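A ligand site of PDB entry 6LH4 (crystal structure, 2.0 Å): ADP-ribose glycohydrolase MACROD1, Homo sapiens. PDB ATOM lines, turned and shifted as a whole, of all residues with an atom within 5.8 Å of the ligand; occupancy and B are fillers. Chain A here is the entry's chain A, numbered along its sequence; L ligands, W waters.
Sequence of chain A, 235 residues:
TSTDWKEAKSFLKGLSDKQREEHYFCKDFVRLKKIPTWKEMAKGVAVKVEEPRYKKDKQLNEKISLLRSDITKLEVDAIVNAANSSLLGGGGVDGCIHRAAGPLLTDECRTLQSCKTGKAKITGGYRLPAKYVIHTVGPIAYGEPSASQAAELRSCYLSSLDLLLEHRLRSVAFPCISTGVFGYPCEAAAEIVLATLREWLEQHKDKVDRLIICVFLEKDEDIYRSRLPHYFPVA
An oxygen (O2) of the ligand sits at hydrogen-bond distance from the backbone NH of Gly 180 (2.8 Å).
N of Val 181 lies within hydrogen-bond range of O1 of the ligand (2.8 Å).
An oxygen (O8) of the ligand lies within hydrogen-bond range of the side-chain hydroxyl of Thr 179 (3.3 Å).
The backbone NH of Thr 179 sits at hydrogen-bond distance from an oxygen (O2) of the ligand (3.4 Å).
O6 of the ligand sits at hydrogen-bond distance from N of Ser 178 (2.8 Å).
An oxygen (O7) of the ligand sits at hydrogen-bond distance from the side-chain amide nitrogen (ND2) of Asn 84 (3.0 Å).
N of Phe 182 sits at hydrogen-bond distance from O2 of the ligand (3.0 Å).
N1 of the ligand sits at hydrogen-bond distance from N of Ile 71, 2.9 Å away.
An oxygen (O7) of the ligand sits at hydrogen-bond distance from the side-chain carboxylate of Asp 94, 2.8 Å away.
SG of Cys 96 lies within hydrogen-bond range of N3 of the ligand (3.3 Å).
An oxygen (O3) of the ligand is in hydrogen-bond range of the backbone NH (N) of Gly 91, at 3.2 Å.
O of Gly 89 sits at hydrogen-bond distance from O7 of the ligand (3.3 Å).
The backbone NH of Gly 92 sits at hydrogen-bond distance from an oxygen (O3) of the ligand (2.9 Å).
The side-chain carboxylate (OD1) of Asp 70 is in hydrogen-bond range of a nitrogen (N3) of the ligand, 3.2 Å away.
The backbone NH (N) of Val 93 sits at hydrogen-bond distance from an oxygen (O5) of the ligand, at 2.9 Å.
OD2 of Asp 94 sits at hydrogen-bond distance from ND2 of Asn 84 (3.5 Å).
OG1 of Thr 179 lies within hydrogen-bond range of O of Cys 176.
The backbone NH of Gly 89 lies close to the side-chain carboxylate of Asp 94 (3.4 Å).
The side-chain carboxylate (OD1) of Asp 70 sits at hydrogen-bond distance from the side-chain hydroxyl (OG1) of Thr 72 (2.8 Å).
The side-chain amide nitrogen of Asn 84 lies within hydrogen-bond range of the backbone carbonyl oxygen of Gly 89 (2.8 Å).
The backbone NH (N) of Ser 69 sits at hydrogen-bond distance from the backbone carbonyl oxygen (O) of Val 215, at 3.0 Å.
N of Gly 183 is in hydrogen-bond range of O of Ser 178, at 3.0 Å.
The backbone carbonyl oxygen (O) of Ser 69 is in hydrogen-bond range of the side-chain sulfur (SG) of Cys 214 (3.0 Å).
Residues that only touch the ligand: Ser 69 (3.8 Å), Ala 82 (3.5 Å), Ala 83 (3.7 Å), Gly 90 (3.4 Å), Cys 176 (3.4 Å), Phe 216 (3.5 Å), Leu 217 (3.7 Å) and Asp 220 (3.8 Å).
22 residues have an atom within 4 Å of the ligand: Ser 69, Asp 70, Ile 71, Ala 82, Ala 83, Asn 84, Gly 89, Gly 90, Gly 91, Gly 92, Val 93, Asp 94, Cys 96, Cys 176, Ser 178, Thr 179, Gly 180, Val 181, Phe 182, Phe 216, Leu 217 and Asp 220.
The nearest printed residue that does not touch the ligand is Ile 177 (4.01 Å).
Water W3 lies within hydrogen-bond range of an oxygen (O8) of the ligand (2.5 Å), the side-chain carboxylate (OD2) of Asp 220 (2.7 Å) and the side-chain hydroxyl (OG1) of Thr 179 (2.8 Å).
Water W9 lies within hydrogen-bond range of O of Ala 82, O5 of the ligand, N of Asp 94 and N of Val 93.
Water W5 lies within hydrogen-bond range of N4 of the ligand (2.8 Å) and SG of Cys 96 (3.2 Å).
Water W1 lies within hydrogen-bond range of O6 of the ligand (2.8 Å), O of Ala 83 (3.0 Å) and N of Gly 138 (3.1 Å).
Water W4 lies within hydrogen-bond range of O of Cys 214 (2.8 Å), N of Cys 176 (2.9 Å) and N2 of the ligand (3.0 Å).
Water W8 lies within hydrogen-bond range of N of Phe 216 (2.7 Å), OD2 of Asp 220 (2.8 Å), N of Leu 217 (3.1 Å), O8 of the ligand (3.1 Å) and SG of Cys 176 (3.6 Å).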
ATOM      1  N   SER A  69     -31.098 -29.253  17.618  1.00  0.00           N
ATOM      2  CA  SER A  69     -31.783 -29.456  18.888  1.00  0.00           C
ATOM      3  C   SER A  69     -30.861 -29.066  20.028  1.00  0.00           C
ATOM      4  O   SER A  69     -29.626 -28.997  19.872  1.00  0.00           O
ATOM      5  CB  SER A  69     -32.246 -30.911  19.063  1.00  0.00           C
ATOM      6  OG  SER A  69     -32.997 -31.080  20.249  1.00  0.00           O
ATOM      7  N   ASP A  70     -31.482 -28.738  21.153  1.00  0.00           N
ATOM      8  CA  ASP A  70     -30.819 -28.726  22.441  1.00  0.00           C
ATOM      9  C   ASP A  70     -30.335 -30.127  22.729  1.00  0.00           C
ATOM     10  O   ASP A  70     -31.131 -31.076  22.730  1.00  0.00           O
ATOM     11  CB  ASP A  70     -31.823 -28.220  23.512  1.00  0.00           C
ATOM     12  CG  ASP A  70     -31.233 -28.106  24.901  1.00  0.00           C
ATOM     13  OD1 ASP A  70     -30.227 -28.792  25.223  1.00  0.00           O
ATOM     14  OD2 ASP A  70     -31.800 -27.342  25.723  1.00  0.00           O
ATOM     15  N   ILE A  71     -29.026 -30.303  22.910  1.00  0.00           N
ATOM     16  CA  ILE A  71     -28.506 -31.668  22.979  1.00  0.00           C
ATOM     17  C   ILE A  71     -28.931 -32.366  24.255  1.00  0.00           C
ATOM     18  O   ILE A  71     -28.940 -33.599  24.294  1.00  0.00           O
ATOM     19  CB  ILE A  71     -26.968 -31.695  22.835  1.00  0.00           C
ATOM     20  CG1 ILE A  71     -26.476 -33.119  22.507  1.00  0.00           C
ATOM     21  CG2 ILE A  71     -26.281 -31.198  24.063  1.00  0.00           C
ATOM     22  CD1 ILE A  71     -24.980 -33.172  22.211  1.00  0.00           C
ATOM     23  N   THR A  72     -29.301 -31.605  25.298  1.00  0.00           N
ATOM     24  CA  THR A  72     -29.681 -32.248  26.555  1.00  0.00           C
ATOM     25  C   THR A  72     -30.988 -33.008  26.440  1.00  0.00           C
ATOM     26  O   THR A  72     -31.288 -33.822  27.307  1.00  0.00           O
ATOM     27  CB  THR A  72     -29.780 -31.218  27.697  1.00  0.00           C
ATOM     28  OG1 THR A  72     -30.870 -30.325  27.428  1.00  0.00           O
ATOM     29  CG2 THR A  72     -28.505 -30.421  27.818  1.00  0.00           C
ATOM     30  N   ALA A  82     -18.769 -30.258  25.129  1.00  0.00           N
ATOM     31  CA  ALA A  82     -17.654 -29.376  24.791  1.00  0.00           C
ATOM     32  C   ALA A  82     -17.128 -28.749  26.076  1.00  0.00           C
ATOM     33  O   ALA A  82     -17.510 -27.644  26.454  1.00  0.00           O
ATOM     34  CB  ALA A  82     -18.093 -28.319  23.794  1.00  0.00           C
ATOM     35  N   ALA A  83     -16.239 -29.470  26.772  1.00  0.00           N
ATOM     36  CA  ALA A  83     -15.873 -29.135  28.147  1.00  0.00           C
ATOM     37  C   ALA A  83     -14.663 -28.197  28.209  1.00  0.00           C
ATOM     38  O   ALA A  83     -14.145 -27.752  27.177  1.00  0.00           O
ATOM     39  CB  ALA A  83     -15.581 -30.404  28.940  1.00  0.00           C
ATOM     40  N   ASN A  84     -14.215 -27.867  29.421  1.00  0.00           N
ATOM     41  CA  ASN A  84     -12.904 -27.252  29.599  1.00  0.00           C
ATOM     42  C   ASN A  84     -11.981 -28.229  30.335  1.00  0.00           C
ATOM     43  O   ASN A  84     -12.435 -29.231  30.917  1.00  0.00           O
ATOM     44  CB  ASN A  84     -13.014 -25.943  30.378  1.00  0.00           C
ATOM     45  CG  ASN A  84     -13.656 -26.135  31.716  1.00  0.00           C
ATOM     46  OD1 ASN A  84     -13.010 -26.614  32.655  1.00  0.00           O
ATOM     47  ND2 ASN A  84     -14.932 -25.828  31.800  1.00  0.00           N
ATOM     48  N   GLY A  89     -17.479 -26.898  34.002  1.00  0.00           N
ATOM     49  CA  GLY A  89     -18.675 -26.311  33.412  1.00  0.00           C
ATOM     50  C   GLY A  89     -18.338 -24.966  32.780  1.00  0.00           C
ATOM     51  O   GLY A  89     -17.209 -24.507  32.810  1.00  0.00           O
ATOM     52  N   GLY A  90     -19.346 -24.339  32.196  1.00  0.00           N
ATOM     53  CA  GLY A  90     -19.101 -23.072  31.541  1.00  0.00           C
ATOM     54  C   GLY A  90     -20.373 -22.565  30.889  1.00  0.00           C
ATOM     55  O   GLY A  90     -21.429 -23.143  31.063  1.00  0.00           O
ATOM     56  N   GLY A  91     -20.233 -21.499  30.098  1.00  0.00           N
ATOM     57  CA  GLY A  91     -21.382 -20.844  29.509  1.00  0.00           C
ATOM     58  C   GLY A  91     -21.898 -21.373  28.184  1.00  0.00           C
ATOM     59  O   GLY A  91     -22.919 -20.885  27.689  1.00  0.00           O
ATOM     60  N   GLY A  92     -21.236 -22.360  27.583  1.00  0.00           N
ATOM     61  CA  GLY A  92     -21.750 -22.923  26.332  1.00  0.00           C
ATOM     62  C   GLY A  92     -22.656 -24.100  26.618  1.00  0.00           C
ATOM     63  O   GLY A  92     -23.435 -24.079  27.565  1.00  0.00           O
ATOM     64  N   VAL A  93     -22.546 -25.143  25.796  1.00  0.00           N
ATOM     65  CA  VAL A  93     -23.339 -26.346  25.997  1.00  0.00           C
ATOM     66  C   VAL A  93     -22.935 -27.067  27.273  1.00  0.00           C
ATOM     67  O   VAL A  93     -23.748 -27.797  27.862  1.00  0.00           O
ATOM     68  CB  VAL A  93     -23.219 -27.260  24.745  1.00  0.00           C
ATOM     69  CG1 VAL A  93     -21.778 -27.699  24.536  1.00  0.00           C
ATOM     70  CG2 VAL A  93     -24.159 -28.458  24.857  1.00  0.00           C
ATOM     71  N   ASP A  94     -21.696 -26.865  27.726  1.00  0.00           N
ATOM     72  CA  ASP A  94     -21.249 -27.373  29.019  1.00  0.00           C
ATOM     73  C   ASP A  94     -22.189 -26.898  30.138  1.00  0.00           C
ATOM     74  O   ASP A  94     -22.571 -27.676  31.028  1.00  0.00           O
ATOM     75  CB  ASP A  94     -19.808 -26.882  29.227  1.00  0.00           C
ATOM     76  CG  ASP A  94     -19.039 -27.617  30.309  1.00  0.00           C
ATOM     77  OD1 ASP A  94     -19.552 -28.595  30.848  1.00  0.00           O
ATOM     78  OD2 ASP A  94     -17.914 -27.186  30.613  1.00  0.00           O
ATOM     79  N   GLY A  95     -22.606 -25.639  30.071  1.00  0.00           N
ATOM     80  CA  GLY A  95     -23.516 -25.122  31.092  1.00  0.00           C
ATOM     81  C   GLY A  95     -24.892 -25.752  30.988  1.00  0.00           C
ATOM     82  O   GLY A  95     -25.503 -26.088  32.009  1.00  0.00           O
ATOM     83  N   CYS A  96     -25.400 -25.934  29.760  1.00  0.00           N
ATOM     84  CA  CYS A  96     -26.693 -26.586  29.593  1.00  0.00           C
ATOM     85  C   CYS A  96     -26.652 -28.006  30.118  1.00  0.00           C
ATOM     86  O   CYS A  96     -27.608 -28.473  30.761  1.00  0.00           O
ATOM     87  CB  CYS A  96     -27.097 -26.579  28.116  1.00  0.00           C
ATOM     88  SG  CYS A  96     -27.220 -24.953  27.393  1.00  0.00           S
ATOM     89  N   GLY A 138     -11.904 -29.294  23.294  1.00  0.00           N
ATOM     90  CA  GLY A 138     -11.476 -28.864  21.996  1.00  0.00           C
ATOM     91  C   GLY A 138     -10.327 -27.869  22.023  1.00  0.00           C
ATOM     92  O   GLY A 138     -10.018 -27.262  23.056  1.00  0.00           O
ATOM     93  N   PRO A 175     -22.052 -32.028  20.001  1.00  0.00           N
ATOM     94  CA  PRO A 175     -22.292 -30.622  19.707  1.00  0.00           C
ATOM     95  C   PRO A 175     -21.192 -30.107  18.798  1.00  0.00           C
ATOM     96  O   PRO A 175     -20.275 -30.855  18.439  1.00  0.00           O
ATOM     97  CB  PRO A 175     -22.253 -29.976  21.107  1.00  0.00           C
ATOM     98  CG  PRO A 175     -21.091 -30.756  21.777  1.00  0.00           C
ATOM     99  CD  PRO A 175     -21.093 -32.181  21.111  1.00  0.00           C
ATOM    100  N   CYS A 176     -21.248 -28.826  18.429  1.00  0.00           N
ATOM    101  CA  CYS A 176     -20.290 -28.282  17.479  1.00  0.00           C
ATOM    102  C   CYS A 176     -19.014 -27.845  18.212  1.00  0.00           C
ATOM    103  O   CYS A 176     -18.647 -26.666  18.222  1.00  0.00           O
ATOM    104  CB  CYS A 176     -20.910 -27.104  16.732  1.00  0.00           C
ATOM    105  SG  CYS A 176     -22.220 -27.669  15.572  1.00  0.00           S
ATOM    106  N   ILE A 177     -18.340 -28.823  18.802  1.00  0.00           N
ATOM    107  CA  ILE A 177     -17.124 -28.610  19.586  1.00  0.00           C
ATOM    108  C   ILE A 177     -16.211 -27.518  19.051  1.00  0.00           C
ATOM    109  O   ILE A 177     -15.869 -27.499  17.861  1.00  0.00           O
ATOM    110  CB  ILE A 177     -16.364 -29.936  19.679  1.00  0.00           C
ATOM    111  CG1 ILE A 177     -17.251 -30.982  20.329  1.00  0.00           C
ATOM    112  CG2 ILE A 177     -15.038 -29.761  20.426  1.00  0.00           C
ATOM    113  CD1 ILE A 177     -16.649 -32.337  20.400  1.00  0.00           C
ATOM    114  N   SER A 178     -15.804 -26.608  19.957  1.00  0.00           N
ATOM    115  CA  SER A 178     -14.787 -25.578  19.772  1.00  0.00           C
ATOM    116  C   SER A 178     -15.316 -24.370  19.023  1.00  0.00           C
ATOM    117  O   SER A 178     -14.609 -23.361  18.942  1.00  0.00           O
ATOM    118  CB  SER A 178     -13.521 -26.072  19.031  1.00  0.00           C
ATOM    119  OG  SER A 178     -12.576 -26.688  19.909  1.00  0.00           O
ATOM    120  N   THR A 179     -16.508 -24.424  18.432  1.00  0.00           N
ATOM    121  CA  THR A 179     -16.962 -23.335  17.578  1.00  0.00           C
ATOM    122  C   THR A 179     -17.666 -22.222  18.339  1.00  0.00           C
ATOM    123  O   THR A 179     -18.004 -21.209  17.719  1.00  0.00           O
ATOM    124  CB  THR A 179     -17.904 -23.857  16.486  1.00  0.00           C
ATOM    125  OG1 THR A 179     -19.092 -24.405  17.079  1.00  0.00           O
ATOM    126  CG2 THR A 179     -17.216 -24.904  15.587  1.00  0.00           C
ATOM    127  N   GLY A 180     -17.898 -22.388  19.631  1.00  0.00           N
ATOM    128  CA  GLY A 180     -18.510 -21.352  20.447  1.00  0.00           C
ATOM    129  C   GLY A 180     -17.457 -20.526  21.152  1.00  0.00           C
ATOM    130  O   GLY A 180     -16.706 -19.800  20.485  1.00  0.00           O
ATOM    131  N   VAL A 181     -17.363 -20.662  22.480  1.00  0.00           N
ATOM    132  CA  VAL A 181     -16.375 -19.914  23.275  1.00  0.00           C
ATOM    133  C   VAL A 181     -14.958 -20.105  22.757  1.00  0.00           C
ATOM    134  O   VAL A 181     -14.133 -19.191  22.839  1.00  0.00           O
ATOM    135  CB  VAL A 181     -16.498 -20.305  24.770  1.00  0.00           C
ATOM    136  CG1 VAL A 181     -15.479 -19.563  25.624  1.00  0.00           C
ATOM    137  CG2 VAL A 181     -17.897 -20.041  25.286  1.00  0.00           C
ATOM    138  N   PHE A 182     -14.634 -21.297  22.223  1.00  0.00           N
ATOM    139  CA  PHE A 182     -13.270 -21.550  21.782  1.00  0.00           C
ATOM    140  C   PHE A 182     -12.994 -21.015  20.372  1.00  0.00           C
ATOM    141  O   PHE A 182     -11.845 -21.075  19.931  1.00  0.00           O
ATOM    142  CB  PHE A 182     -12.954 -23.046  21.866  1.00  0.00           C
ATOM    143  CG  PHE A 182     -12.614 -23.520  23.267  1.00  0.00           C
ATOM    144  CD1 PHE A 182     -12.656 -22.637  24.365  1.00  0.00           C
ATOM    145  CD2 PHE A 182     -12.257 -24.849  23.513  1.00  0.00           C
ATOM    146  CE1 PHE A 182     -12.334 -23.058  25.656  1.00  0.00           C
ATOM    147  CE2 PHE A 182     -11.934 -25.286  24.799  1.00  0.00           C
ATOM    148  CZ  PHE A 182     -11.976 -24.387  25.879  1.00  0.00           C
ATOM    149  N   GLY A 183     -13.996 -20.488  19.684  1.00  0.00           N
ATOM    150  CA  GLY A 183     -13.751 -19.685  18.493  1.00  0.00           C
ATOM    151  C   GLY A 183     -13.214 -20.395  17.248  1.00  0.00           C
ATOM    152  O   GLY A 183     -12.484 -19.768  16.467  1.00  0.00           O
ATOM    153  N   CYS A 214     -25.520 -32.871  16.405  1.00  0.00           N
ATOM    154  CA  CYS A 214     -26.566 -32.064  17.036  1.00  0.00           C
ATOM    155  C   CYS A 214     -26.104 -30.624  16.924  1.00  0.00           C
ATOM    156  O   CYS A 214     -25.188 -30.194  17.633  1.00  0.00           O
ATOM    157  CB  CYS A 214     -26.809 -32.499  18.484  1.00  0.00           C
ATOM    158  SG  CYS A 214     -28.203 -31.590  19.266  1.00  0.00           S
ATOM    159  N   VAL A 215     -26.667 -29.901  15.979  1.00  0.00           N
ATOM    160  CA  VAL A 215     -26.318 -28.497  15.784  1.00  0.00           C
ATOM    161  C   VAL A 215     -27.314 -27.673  16.585  1.00  0.00           C
ATOM    162  O   VAL A 215     -28.392 -28.149  16.947  1.00  0.00           O
ATOM    163  CB  VAL A 215     -26.312 -28.076  14.302  1.00  0.00           C
ATOM    164  CG1 VAL A 215     -25.248 -28.872  13.501  1.00  0.00           C
ATOM    165  CG2 VAL A 215     -27.667 -28.233  13.673  1.00  0.00           C
ATOM    166  N   PHE A 216     -26.964 -26.428  16.848  1.00  0.00           N
ATOM    167  CA  PHE A 216     -27.776 -25.559  17.685  1.00  0.00           C
ATOM    168  C   PHE A 216     -28.148 -24.258  16.987  1.00  0.00           C
ATOM    169  O   PHE A 216     -29.309 -23.839  17.031  1.00  0.00           O
ATOM    170  CB  PHE A 216     -27.039 -25.262  18.993  1.00  0.00           C
ATOM    171  CG  PHE A 216     -27.889 -24.629  20.042  1.00  0.00           C
ATOM    172  CD1 PHE A 216     -28.886 -25.358  20.679  1.00  0.00           C
ATOM    173  CD2 PHE A 216     -27.693 -23.309  20.400  1.00  0.00           C
ATOM    174  CE1 PHE A 216     -29.670 -24.772  21.670  1.00  0.00           C
ATOM    175  CE2 PHE A 216     -28.470 -22.717  21.391  1.00  0.00           C
ATOM    176  CZ  PHE A 216     -29.463 -23.450  22.019  1.00  0.00           C
ATOM    177  N   LEU A 217     -27.183 -23.615  16.330  1.00  0.00           N
ATOM    178  CA  LEU A 217     -27.467 -22.463  15.510  1.00  0.00           C
ATOM    179  C   LEU A 217     -27.891 -22.884  14.104  1.00  0.00           C
ATOM    180  O   LEU A 217     -27.428 -23.899  13.569  1.00  0.00           O
ATOM    181  CB  LEU A 217     -26.255 -21.544  15.420  1.00  0.00           C
ATOM    182  CG  LEU A 217     -25.416 -21.398  16.668  1.00  0.00           C
ATOM    183  CD1 LEU A 217     -24.123 -20.697  16.288  1.00  0.00           C
ATOM    184  CD2 LEU A 217     -26.182 -20.600  17.724  1.00  0.00           C
ATOM    185  N   ASP A 220     -24.809 -23.369  11.714  1.00  0.00           N
ATOM    186  CA  ASP A 220     -24.219 -24.693  11.596  1.00  0.00           C
ATOM    187  C   ASP A 220     -25.156 -25.672  10.917  1.00  0.00           C
ATOM    188  O   ASP A 220     -24.708 -26.543  10.167  1.00  0.00           O
ATOM    189  CB  ASP A 220     -23.796 -25.235  12.952  1.00  0.00           C
ATOM    190  CG  ASP A 220     -22.725 -24.398  13.590  1.00  0.00           C
ATOM    191  OD1 ASP A 220     -21.631 -24.298  12.981  1.00  0.00           O
ATOM    192  OD2 ASP A 220     -22.995 -23.802  14.659  1.00  0.00           O
HETATM  193  N1  LIG L   1     -27.283 -27.993  22.891  1.00  0.00           N
HETATM  194  C1  LIG L   1     -26.514 -28.187  21.820  1.00  0.00           C
HETATM  195  N2  LIG L   1     -25.573 -27.408  21.314  1.00  0.00           N
HETATM  196  C2  LIG L   1     -25.437 -26.299  22.048  1.00  0.00           C
HETATM  197  C3  LIG L   1     -26.141 -25.965  23.175  1.00  0.00           C
HETATM  198  C4  LIG L   1     -27.124 -26.865  23.603  1.00  0.00           C
HETATM  199  N3  LIG L   1     -27.871 -26.681  24.675  1.00  0.00           N
HETATM  200  N4  LIG L   1     -25.704 -24.746  23.651  1.00  0.00           N
HETATM  201  C5  LIG L   1     -24.772 -24.374  22.823  1.00  0.00           C
HETATM  202  N5  LIG L   1     -24.564 -25.269  21.824  1.00  0.00           N
HETATM  203  P1  LIG L   1     -19.410 -23.996  23.145  1.00  0.00           P
HETATM  204  P2  LIG L   1     -16.549 -24.555  22.800  1.00  0.00           P
HETATM  205  C6  LIG L   1     -23.585 -25.186  20.768  1.00  0.00           C
HETATM  206  O1  LIG L   1     -19.098 -22.597  23.396  1.00  0.00           O
HETATM  207  O2  LIG L   1     -16.492 -23.606  21.697  1.00  0.00           O
HETATM  208  C7  LIG L   1     -17.594 -23.958  27.435  1.00  0.00           C
HETATM  209  O3  LIG L   1     -18.620 -23.486  28.135  1.00  0.00           O
HETATM  210  C8  LIG L   1     -23.134 -23.793  20.420  1.00  0.00           C
HETATM  211  O4  LIG L   1     -24.119 -23.144  19.675  1.00  0.00           O
HETATM  212  O5  LIG L   1     -20.386 -24.705  23.951  1.00  0.00           O
HETATM  213  O6  LIG L   1     -15.889 -25.837  22.678  1.00  0.00           O
HETATM  214  C9  LIG L   1     -16.579 -24.813  28.211  1.00  0.00           C
HETATM  215  O7  LIG L   1     -16.695 -24.853  29.605  1.00  0.00           O
HETATM  216  C10 LIG L   1     -21.831 -24.081  19.673  1.00  0.00           C
HETATM  217  O8  LIG L   1     -22.156 -24.293  18.318  1.00  0.00           O
HETATM  218  O9  LIG L   1     -18.064 -24.775  23.194  1.00  0.00           O
HETATM  219  C11 LIG L   1     -15.222 -24.296  27.771  1.00  0.00           C
HETATM  220  O10 LIG L   1     -14.640 -23.392  28.674  1.00  0.00           O
HETATM  221  C12 LIG L   1     -21.361 -25.405  20.268  1.00  0.00           C
HETATM  222  O11 LIG L   1     -22.407 -25.798  21.179  1.00  0.00           O
HETATM  223  C13 LIG L   1     -15.618 -23.599  26.474  1.00  0.00           C
HETATM  224  O12 LIG L   1     -16.881 -22.999  26.782  1.00  0.00           O
HETATM  225  C14 LIG L   1     -20.062 -25.370  21.019  1.00  0.00           C
HETATM  226  O13 LIG L   1     -19.917 -24.100  21.655  1.00  0.00           O
HETATM  227  C15 LIG L   1     -15.756 -24.549  25.305  1.00  0.00           C
HETATM  228  O14 LIG L   1     -16.017 -23.828  24.092  1.00  0.00           O
HETATM  229  O   HOH W   1     -14.513 -27.840  24.151  1.00  0.00           O
HETATM  230  O   HOH W   2     -23.612 -21.266  23.422  1.00  0.00           O
HETATM  231  O   HOH W   3     -21.323 -22.817  16.493  1.00  0.00           O
HETATM  232  O   HOH W   4     -23.958 -27.965  18.791  1.00  0.00           O
HETATM  233  O   HOH W   5     -26.984 -22.717  25.144  1.00  0.00           O
HETATM  234  O   HOH W   6     -21.029 -20.701  23.073  1.00  0.00           O
HETATM  235  O   HOH W   7     -24.599 -20.512  20.994  1.00  0.00           O
HETATM  236  O   HOH W   8     -24.568 -25.175  16.574  1.00  0.00           O
HETATM  237  O   HOH W   9     -19.447 -26.020  26.073  1.00  0.00           O
